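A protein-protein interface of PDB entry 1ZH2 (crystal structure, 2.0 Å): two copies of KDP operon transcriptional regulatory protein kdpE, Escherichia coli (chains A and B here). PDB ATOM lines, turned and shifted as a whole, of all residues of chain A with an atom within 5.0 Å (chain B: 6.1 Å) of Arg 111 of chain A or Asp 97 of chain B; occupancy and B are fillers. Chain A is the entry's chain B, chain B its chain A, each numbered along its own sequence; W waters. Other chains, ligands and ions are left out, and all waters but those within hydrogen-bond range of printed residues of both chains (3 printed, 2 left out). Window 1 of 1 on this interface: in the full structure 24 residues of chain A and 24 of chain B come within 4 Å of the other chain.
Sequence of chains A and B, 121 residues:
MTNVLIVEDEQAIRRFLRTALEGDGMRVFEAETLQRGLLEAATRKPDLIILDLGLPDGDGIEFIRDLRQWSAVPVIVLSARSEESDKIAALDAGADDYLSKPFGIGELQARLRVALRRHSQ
The side-chain carboxylate (OD1) of Asp 97 of chain B is in salt-bridge range of the guanidinium group (NH1) of Arg 111 of chain A (2.9 Å). O of Tyr 98 of chain B sits at hydrogen-bond distance from NH2 of Arg 111 of chain A, 3.2 Å away. The guanidinium group (NH1) of Arg 111 of chain B lies within salt-bridge range of the side-chain carboxylate (OD1) of Asp 97 of chain A.
The backbone NH (N) of Asp 96 of chain B lies within hydrogen-bond range of the backbone carbonyl oxygen (O) of Val 75 of chain B (2.8 Å). The backbone carbonyl oxygen (O) of Val 75 of chain B sits at hydrogen-bond distance from the backbone NH (N) of Asp 97 of chain B, 3.4 Å away. N of Val 77 of chain B lies within hydrogen-bond range of O of Asp 97 of chain B. O of Ala 90 of chain B sits at hydrogen-bond distance from N of Ala 95 of chain B (3.1 Å). The side-chain carboxylate of Asp 97 of chain B lies within salt-bridge range of the guanidinium group of Arg 111 of chain B (2.8 Å). The side-chain carboxylate of Glu 107 of chain A is in salt-bridge range of the guanidinium group of Arg 111 of chain A, at 2.9 Å.
Among the printed residues, merely in contact across the chains: Glu 107 of chain A with Lys 87 of chain B (3.6 Å), Arg 111 of chain A with Leu 91 of chain B (3.5 Å), Val 114 of chain A with Ala 95 of chain B (3.8 Å) and Val 114 of chain A with Asp 96 of chain B (3.6 Å).
Printed residues of chain B within 4 Å of Glu 107 of chain A: Lys 87. Printed residues of chain B within 4 Å of Arg 111 of chain A: Leu 91, Asp 97 and Tyr 98. Arg 113 of chain A touches none of the printed residues of chain B. Ala 90 of chain B touches none of the printed residues of chain A. Of the printed residues of chain A, Leu 91 of chain B touches Arg 111. Of the printed residues of chain A, Asp 96 of chain B touches Val 114. Of chain A, only Arg 111 (2.9 Å) comes within 4 Å of Asp 97 of chain B. Of the printed residues of chain A, Tyr 98 of chain B touches Arg 111. Of the printed residues of chain A, Arg 111 of chain B touches Asp 97 (3.0 Å). The nearest residue of chain B that does not touch Arg 111 of chain A is Arg 111 of chain B (4.3 Å). The nearest printed residue of chain A that does not touch Arg 111 of chain B is Arg 111 of chain A (4.3 Å).
Printed residues of chain B that touch a printed residue of chain A: Lys 87, Leu 91, Ala 95, Asp 96, Asp 97, Tyr 98 and Arg 111. Hydrophobic or aromatic side chains of chain B that line the printed part of chain A: Leu 91 and Tyr 98.
Asp 97 of chain A touches Arg 111 of chain B, and with the chains exchanged Arg 111 of chain A touches Asp 97 of chain B. Positions printed for both chains: 76, 97, 99 and 111. Of the 7 pairs that touch across the chains among the printed residues, 2 have their exchanged pair printed and touching as well.
Water W2 lies within hydrogen-bond range of O of Tyr 98 of chain B (2.5 Å), OD1 of Asp 97 of chain B (2.9 Å), NH1 of Arg 111 of chain B (3.2 Å) and NH2 of Arg 111 of chain A (3.2 Å). Water W1 lies within hydrogen-bond range of OD1 of Asp 97 of chain A, NH1 of Arg 111 of chain A and NH2 of Arg 111 of chain B. Water W3 lies within hydrogen-bond range of the backbone carbonyl oxygen (O) of Ala 110 of chain A (2.9 Å) and the backbone carbonyl oxygen (O) of Leu 91 of chain B (3.5 Å).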
ATOM      1  N   ILE A  76      29.784  35.750  19.249  1.00  0.00           N
ATOM      2  CA  ILE A  76      29.505  34.426  18.690  1.00  0.00           C
ATOM      3  C   ILE A  76      29.565  34.586  17.167  1.00  0.00           C
ATOM      4  O   ILE A  76      28.876  35.452  16.620  1.00  0.00           O
ATOM      5  CB  ILE A  76      28.088  33.943  19.116  1.00  0.00           C
ATOM      6  CG1 ILE A  76      28.063  33.739  20.636  1.00  0.00           C
ATOM      7  CG2 ILE A  76      27.756  32.607  18.373  1.00  0.00           C
ATOM      8  CD1 ILE A  76      26.802  33.090  21.182  1.00  0.00           C
ATOM      9  N   ASP A  97      32.599  31.702  20.376  1.00  0.00           N
ATOM     10  CA  ASP A  97      31.887  30.532  19.881  1.00  0.00           C
ATOM     11  C   ASP A  97      31.767  30.686  18.361  1.00  0.00           C
ATOM     12  O   ASP A  97      31.993  31.778  17.799  1.00  0.00           O
ATOM     13  CB  ASP A  97      30.519  30.382  20.561  1.00  0.00           C
ATOM     14  CG  ASP A  97      30.073  28.940  20.659  1.00  0.00           C
ATOM     15  OD1 ASP A  97      30.477  28.091  19.776  1.00  0.00           O
ATOM     16  OD2 ASP A  97      29.291  28.575  21.585  1.00  0.00           O
ATOM     17  N   LEU A  99      29.369  28.937  15.037  1.00  0.00           N
ATOM     18  CA  LEU A  99      28.309  28.047  14.579  1.00  0.00           C
ATOM     19  C   LEU A  99      28.306  28.018  13.056  1.00  0.00           C
ATOM     20  O   LEU A  99      28.218  29.053  12.406  1.00  0.00           O
ATOM     21  CB  LEU A  99      26.936  28.532  15.069  1.00  0.00           C
ATOM     22  CG  LEU A  99      26.543  28.199  16.511  1.00  0.00           C
ATOM     23  CD1 LEU A  99      27.079  29.284  17.395  1.00  0.00           C
ATOM     24  CD2 LEU A  99      25.019  28.151  16.673  1.00  0.00           C
ATOM     25  N   GLU A 107      19.846  26.096  19.421  1.00  0.00           N
ATOM     26  CA  GLU A 107      21.252  25.999  19.819  1.00  0.00           C
ATOM     27  C   GLU A 107      21.898  27.376  19.931  1.00  0.00           C
ATOM     28  O   GLU A 107      22.618  27.672  20.889  1.00  0.00           O
ATOM     29  CB  GLU A 107      22.065  25.160  18.834  1.00  0.00           C
ATOM     30  CG  GLU A 107      23.440  24.778  19.383  1.00  0.00           C
ATOM     31  CD  GLU A 107      24.233  23.953  18.387  1.00  0.00           C
ATOM     32  OE1 GLU A 107      23.606  23.401  17.462  1.00  0.00           O
ATOM     33  OE2 GLU A 107      25.478  23.886  18.524  1.00  0.00           O
ATOM     34  N   LEU A 108      21.647  28.229  18.962  1.00  0.00           N
ATOM     35  CA  LEU A 108      22.164  29.602  19.062  1.00  0.00           C
ATOM     36  C   LEU A 108      21.755  30.285  20.378  1.00  0.00           C
ATOM     37  O   LEU A 108      22.581  30.893  21.074  1.00  0.00           O
ATOM     38  CB  LEU A 108      21.714  30.415  17.853  1.00  0.00           C
ATOM     39  CG  LEU A 108      22.153  31.879  17.878  1.00  0.00           C
ATOM     40  CD1 LEU A 108      23.702  31.989  18.042  1.00  0.00           C
ATOM     41  CD2 LEU A 108      21.675  32.550  16.592  1.00  0.00           C
ATOM     42  N   GLN A 109      20.476  30.172  20.732  1.00  0.00           N
ATOM     43  CA  GLN A 109      19.964  30.740  21.970  1.00  0.00           C
ATOM     44  C   GLN A 109      20.674  30.186  23.205  1.00  0.00           C
ATOM     45  O   GLN A 109      21.039  30.961  24.114  1.00  0.00           O
ATOM     46  CB  GLN A 109      18.423  30.536  22.085  1.00  0.00           C
ATOM     47  CG  GLN A 109      17.638  31.518  21.226  1.00  0.00           C
ATOM     48  CD  GLN A 109      16.187  31.089  20.926  1.00  0.00           C
ATOM     49  OE1 GLN A 109      15.881  29.885  20.813  1.00  0.00           O
ATOM     50  NE2 GLN A 109      15.301  32.077  20.768  1.00  0.00           N
ATOM     51  N   ALA A 110      20.844  28.862  23.263  1.00  0.00           N
ATOM     52  CA  ALA A 110      21.544  28.261  24.394  1.00  0.00           C
ATOM     53  C   ALA A 110      22.981  28.781  24.467  1.00  0.00           C
ATOM     54  O   ALA A 110      23.494  29.061  25.552  1.00  0.00           O
ATOM     55  CB  ALA A 110      21.514  26.710  24.351  1.00  0.00           C
ATOM     56  N   ARG A 111      23.632  28.901  23.325  1.00  0.00           N
ATOM     57  CA  ARG A 111      24.999  29.390  23.313  1.00  0.00           C
ATOM     58  C   ARG A 111      25.092  30.879  23.686  1.00  0.00           C
ATOM     59  O   ARG A 111      26.057  31.283  24.358  1.00  0.00           O
ATOM     60  CB  ARG A 111      25.681  29.069  21.965  1.00  0.00           C
ATOM     61  CG  ARG A 111      25.946  27.546  21.831  1.00  0.00           C
ATOM     62  CD  ARG A 111      26.523  27.161  20.457  1.00  0.00           C
ATOM     63  NE  ARG A 111      26.796  25.727  20.378  1.00  0.00           N
ATOM     64  CZ  ARG A 111      27.838  25.140  20.934  1.00  0.00           C
ATOM     65  NH1 ARG A 111      28.738  25.866  21.611  1.00  0.00           N
ATOM     66  NH2 ARG A 111      27.990  23.812  20.787  1.00  0.00           N
ATOM     67  N   LEU A 112      24.064  31.643  23.306  1.00  0.00           N
ATOM     68  CA  LEU A 112      23.916  33.051  23.726  1.00  0.00           C
ATOM     69  C   LEU A 112      23.845  33.123  25.244  1.00  0.00           C
ATOM     70  O   LEU A 112      24.500  33.944  25.868  1.00  0.00           O
ATOM     71  CB  LEU A 112      22.604  33.618  23.200  1.00  0.00           C
ATOM     72  CG  LEU A 112      22.652  34.717  22.186  1.00  0.00           C
ATOM     73  CD1 LEU A 112      23.750  34.356  21.222  1.00  0.00           C
ATOM     74  CD2 LEU A 112      21.307  34.806  21.457  1.00  0.00           C
ATOM     75  N   ARG A 113      23.051  32.252  25.847  1.00  0.00           N
ATOM     76  CA  ARG A 113      22.949  32.264  27.299  1.00  0.00           C
ATOM     77  C   ARG A 113      24.297  31.995  27.958  1.00  0.00           C
ATOM     78  O   ARG A 113      24.666  32.683  28.892  1.00  0.00           O
ATOM     79  CB  ARG A 113      21.861  31.318  27.798  1.00  0.00           C
ATOM     80  CG  ARG A 113      20.447  31.741  27.363  1.00  0.00           C
ATOM     81  CD  ARG A 113      19.319  30.916  27.977  1.00  0.00           C
ATOM     82  NE  ARG A 113      19.236  29.526  27.482  1.00  0.00           N
ATOM     83  CZ  ARG A 113      18.552  29.144  26.411  1.00  0.00           C
ATOM     84  NH1 ARG A 113      17.892  30.027  25.676  1.00  0.00           N
ATOM     85  NH2 ARG A 113      18.509  27.868  26.073  1.00  0.00           N
ATOM     86  N   VAL A 114      25.065  31.024  27.471  1.00  0.00           N
ATOM     87  CA  VAL A 114      26.381  30.746  28.070  1.00  0.00           C
ATOM     88  C   VAL A 114      27.218  31.988  28.033  1.00  0.00           C
ATOM     89  O   VAL A 114      27.872  32.352  29.005  1.00  0.00           O
ATOM     90  CB  VAL A 114      27.160  29.583  27.337  1.00  0.00           C
ATOM     91  CG1 VAL A 114      28.606  29.430  27.887  1.00  0.00           C
ATOM     92  CG2 VAL A 114      26.370  28.240  27.444  1.00  0.00           C
ATOM     93  N   ALA A 115      27.210  32.647  26.901  1.00  0.00           N
ATOM     94  CA  ALA A 115      28.128  33.730  26.681  1.00  0.00           C
ATOM     95  C   ALA A 115      27.745  34.903  27.549  1.00  0.00           C
ATOM     96  O   ALA A 115      28.610  35.704  27.866  1.00  0.00           O
ATOM     97  CB  ALA A 115      28.145  34.147  25.198  1.00  0.00           C
ATOM     98  N   VAL B  75      33.531  23.856  31.769  1.00  0.00           N
ATOM     99  CA  VAL B  75      33.364  22.460  31.407  1.00  0.00           C
ATOM    100  C   VAL B  75      33.061  22.416  29.895  1.00  0.00           C
ATOM    101  O   VAL B  75      32.190  23.137  29.421  1.00  0.00           O
ATOM    102  CB  VAL B  75      32.154  21.852  32.136  1.00  0.00           C
ATOM    103  CG1 VAL B  75      31.810  20.494  31.507  1.00  0.00           C
ATOM    104  CG2 VAL B  75      32.457  21.676  33.676  1.00  0.00           C
ATOM    105  N   ILE B  76      33.824  21.622  29.157  1.00  0.00           N
ATOM    106  CA  ILE B  76      33.549  21.358  27.734  1.00  0.00           C
ATOM    107  C   ILE B  76      33.068  19.890  27.651  1.00  0.00           C
ATOM    108  O   ILE B  76      33.757  18.963  28.060  1.00  0.00           O
ATOM    109  CB  ILE B  76      34.807  21.572  26.877  1.00  0.00           C
ATOM    110  CG1 ILE B  76      35.298  23.029  26.991  1.00  0.00           C
ATOM    111  CG2 ILE B  76      34.573  21.113  25.355  1.00  0.00           C
ATOM    112  CD1 ILE B  76      36.318  23.460  25.902  1.00  0.00           C
ATOM    113  N   VAL B  77      31.854  19.703  27.163  1.00  0.00           N
ATOM    114  CA  VAL B  77      31.291  18.387  27.070  1.00  0.00           C
ATOM    115  C   VAL B  77      31.720  17.715  25.766  1.00  0.00           C
ATOM    116  O   VAL B  77      31.809  18.382  24.732  1.00  0.00           O
ATOM    117  CB  VAL B  77      29.729  18.464  27.192  1.00  0.00           C
ATOM    118  CG1 VAL B  77      29.053  17.262  26.554  1.00  0.00           C
ATOM    119  CG2 VAL B  77      29.338  18.596  28.661  1.00  0.00           C
ATOM    120  N   LEU B  78      31.991  16.399  25.860  1.00  0.00           N
ATOM    121  CA  LEU B  78      32.131  15.498  24.700  1.00  0.00           C
ATOM    122  C   LEU B  78      30.973  14.583  24.698  1.00  0.00           C
ATOM    123  O   LEU B  78      30.437  14.165  25.726  1.00  0.00           O
ATOM    124  CB  LEU B  78      33.346  14.542  24.845  1.00  0.00           C
ATOM    125  CG  LEU B  78      34.655  15.342  24.965  1.00  0.00           C
ATOM    126  CD1 LEU B  78      35.861  14.545  24.497  1.00  0.00           C
ATOM    127  CD2 LEU B  78      34.483  16.506  24.103  1.00  0.00           C
ATOM    128  N   LYS B  87      22.656  19.278  23.000  1.00  0.00           N
ATOM    129  CA  LYS B  87      23.537  20.411  23.246  1.00  0.00           C
ATOM    130  C   LYS B  87      22.843  21.436  24.140  1.00  0.00           C
ATOM    131  O   LYS B  87      23.423  21.918  25.126  1.00  0.00           O
ATOM    132  CB  LYS B  87      24.043  21.022  21.932  1.00  0.00           C
ATOM    133  CG  LYS B  87      24.582  19.940  20.960  1.00  0.00           C
ATOM    134  CD  LYS B  87      25.073  20.500  19.640  1.00  0.00           C
ATOM    135  CE  LYS B  87      25.801  19.389  18.810  1.00  0.00           C
ATOM    136  NZ  LYS B  87      26.423  19.897  17.504  1.00  0.00           N
ATOM    137  N   ALA B  90      22.769  20.291  27.945  1.00  0.00           N
ATOM    138  CA  ALA B  90      24.066  20.336  28.615  1.00  0.00           C
ATOM    139  C   ALA B  90      24.519  21.787  28.874  1.00  0.00           C
ATOM    140  O   ALA B  90      25.006  22.133  29.957  1.00  0.00           O
ATOM    141  CB  ALA B  90      25.097  19.582  27.787  1.00  0.00           C
ATOM    142  N   LEU B  91      24.385  22.633  27.857  1.00  0.00           N
ATOM    143  CA  LEU B  91      24.759  24.034  27.996  1.00  0.00           C
ATOM    144  C   LEU B  91      23.897  24.688  29.098  1.00  0.00           C
ATOM    145  O   LEU B  91      24.418  25.336  30.031  1.00  0.00           O
ATOM    146  CB  LEU B  91      24.611  24.720  26.627  1.00  0.00           C
ATOM    147  CG  LEU B  91      25.628  24.244  25.564  1.00  0.00           C
ATOM    148  CD1 LEU B  91      25.462  24.989  24.238  1.00  0.00           C
ATOM    149  CD2 LEU B  91      27.028  24.469  26.092  1.00  0.00           C
ATOM    150  N   ALA B  95      27.307  23.665  31.264  1.00  0.00           N
ATOM    151  CA  ALA B  95      28.502  23.400  30.461  1.00  0.00           C
ATOM    152  C   ALA B  95      28.802  24.681  29.721  1.00  0.00           C
ATOM    153  O   ALA B  95      27.910  25.471  29.464  1.00  0.00           O
ATOM    154  CB  ALA B  95      28.256  22.250  29.477  1.00  0.00           C
ATOM    155  N   ASP B  96      30.070  24.903  29.418  1.00  0.00           N
ATOM    156  CA  ASP B  96      30.504  26.067  28.656  1.00  0.00           C
ATOM    157  C   ASP B  96      30.518  25.822  27.133  1.00  0.00           C
ATOM    158  O   ASP B  96      30.392  26.765  26.344  1.00  0.00           O
ATOM    159  CB  ASP B  96      31.901  26.428  29.114  1.00  0.00           C
ATOM    160  CG  ASP B  96      31.926  26.841  30.572  1.00  0.00           C
ATOM    161  OD1 ASP B  96      31.825  26.030  31.502  1.00  0.00           O
ATOM    162  OD2 ASP B  96      31.988  28.054  30.826  1.00  0.00           O
ATOM    163  N   ASP B  97      30.713  24.565  26.729  1.00  0.00           N
ATOM    164  CA  ASP B  97      30.778  24.259  25.295  1.00  0.00           C
ATOM    165  C   ASP B  97      30.452  22.785  25.144  1.00  0.00           C
ATOM    166  O   ASP B  97      30.359  22.024  26.137  1.00  0.00           O
ATOM    167  CB  ASP B  97      32.185  24.610  24.745  1.00  0.00           C
ATOM    168  CG  ASP B  97      32.181  24.990  23.249  1.00  0.00           C
ATOM    169  OD1 ASP B  97      31.244  24.587  22.495  1.00  0.00           O
ATOM    170  OD2 ASP B  97      33.082  25.712  22.754  1.00  0.00           O
ATOM    171  N   TYR B  98      30.267  22.369  23.901  1.00  0.00           N
ATOM    172  CA  TYR B  98      29.841  21.021  23.606  1.00  0.00           C
ATOM    173  C   TYR B  98      30.372  20.688  22.229  1.00  0.00           C
ATOM    174  O   TYR B  98      30.159  21.458  21.277  1.00  0.00           O
ATOM    175  CB  TYR B  98      28.309  21.023  23.584  1.00  0.00           C
ATOM    176  CG  TYR B  98      27.660  19.669  23.474  1.00  0.00           C
ATOM    177  CD1 TYR B  98      27.888  18.840  22.384  1.00  0.00           C
ATOM    178  CD2 TYR B  98      26.803  19.229  24.461  1.00  0.00           C
ATOM    179  CE1 TYR B  98      27.276  17.612  22.277  1.00  0.00           C
ATOM    180  CE2 TYR B  98      26.195  18.008  24.379  1.00  0.00           C
ATOM    181  CZ  TYR B  98      26.434  17.187  23.295  1.00  0.00           C
ATOM    182  OH  TYR B  98      25.816  15.949  23.237  1.00  0.00           O
ATOM    183  N   LEU B  99      31.039  19.545  22.126  1.00  0.00           N
ATOM    184  CA  LEU B  99      31.542  19.028  20.854  1.00  0.00           C
ATOM    185  C   LEU B  99      31.061  17.610  20.708  1.00  0.00           C
ATOM    186  O   LEU B  99      31.255  16.790  21.618  1.00  0.00           O
ATOM    187  CB  LEU B  99      33.081  19.036  20.830  1.00  0.00           C
ATOM    188  CG  LEU B  99      33.791  20.136  20.047  1.00  0.00           C
ATOM    189  CD1 LEU B  99      35.263  19.769  19.749  1.00  0.00           C
ATOM    190  CD2 LEU B  99      33.086  20.464  18.733  1.00  0.00           C
ATOM    191  N   ARG B 111      38.828  25.637  21.350  1.00  0.00           N
ATOM    192  CA  ARG B 111      37.731  25.854  22.294  1.00  0.00           C
ATOM    193  C   ARG B 111      38.213  25.827  23.753  1.00  0.00           C
ATOM    194  O   ARG B 111      37.704  26.596  24.596  1.00  0.00           O
ATOM    195  CB  ARG B 111      36.607  24.840  22.037  1.00  0.00           C
ATOM    196  CG  ARG B 111      35.862  25.153  20.730  1.00  0.00           C
ATOM    197  CD  ARG B 111      34.722  24.161  20.420  1.00  0.00           C
ATOM    198  NE  ARG B 111      34.100  24.506  19.138  1.00  0.00           N
ATOM    199  CZ  ARG B 111      33.169  25.453  18.969  1.00  0.00           C
ATOM    200  NH1 ARG B 111      32.676  26.128  20.026  1.00  0.00           N
ATOM    201  NH2 ARG B 111      32.658  25.650  17.756  1.00  0.00           N
HETATM  202  O   HOH W   1      29.360  25.976  18.493  1.00  0.00           O
HETATM  203  O   HOH W   2      31.044  23.368  19.896  1.00  0.00           O
HETATM  204  O   HOH W   3      22.934  27.847  28.113  1.00  0.00           O
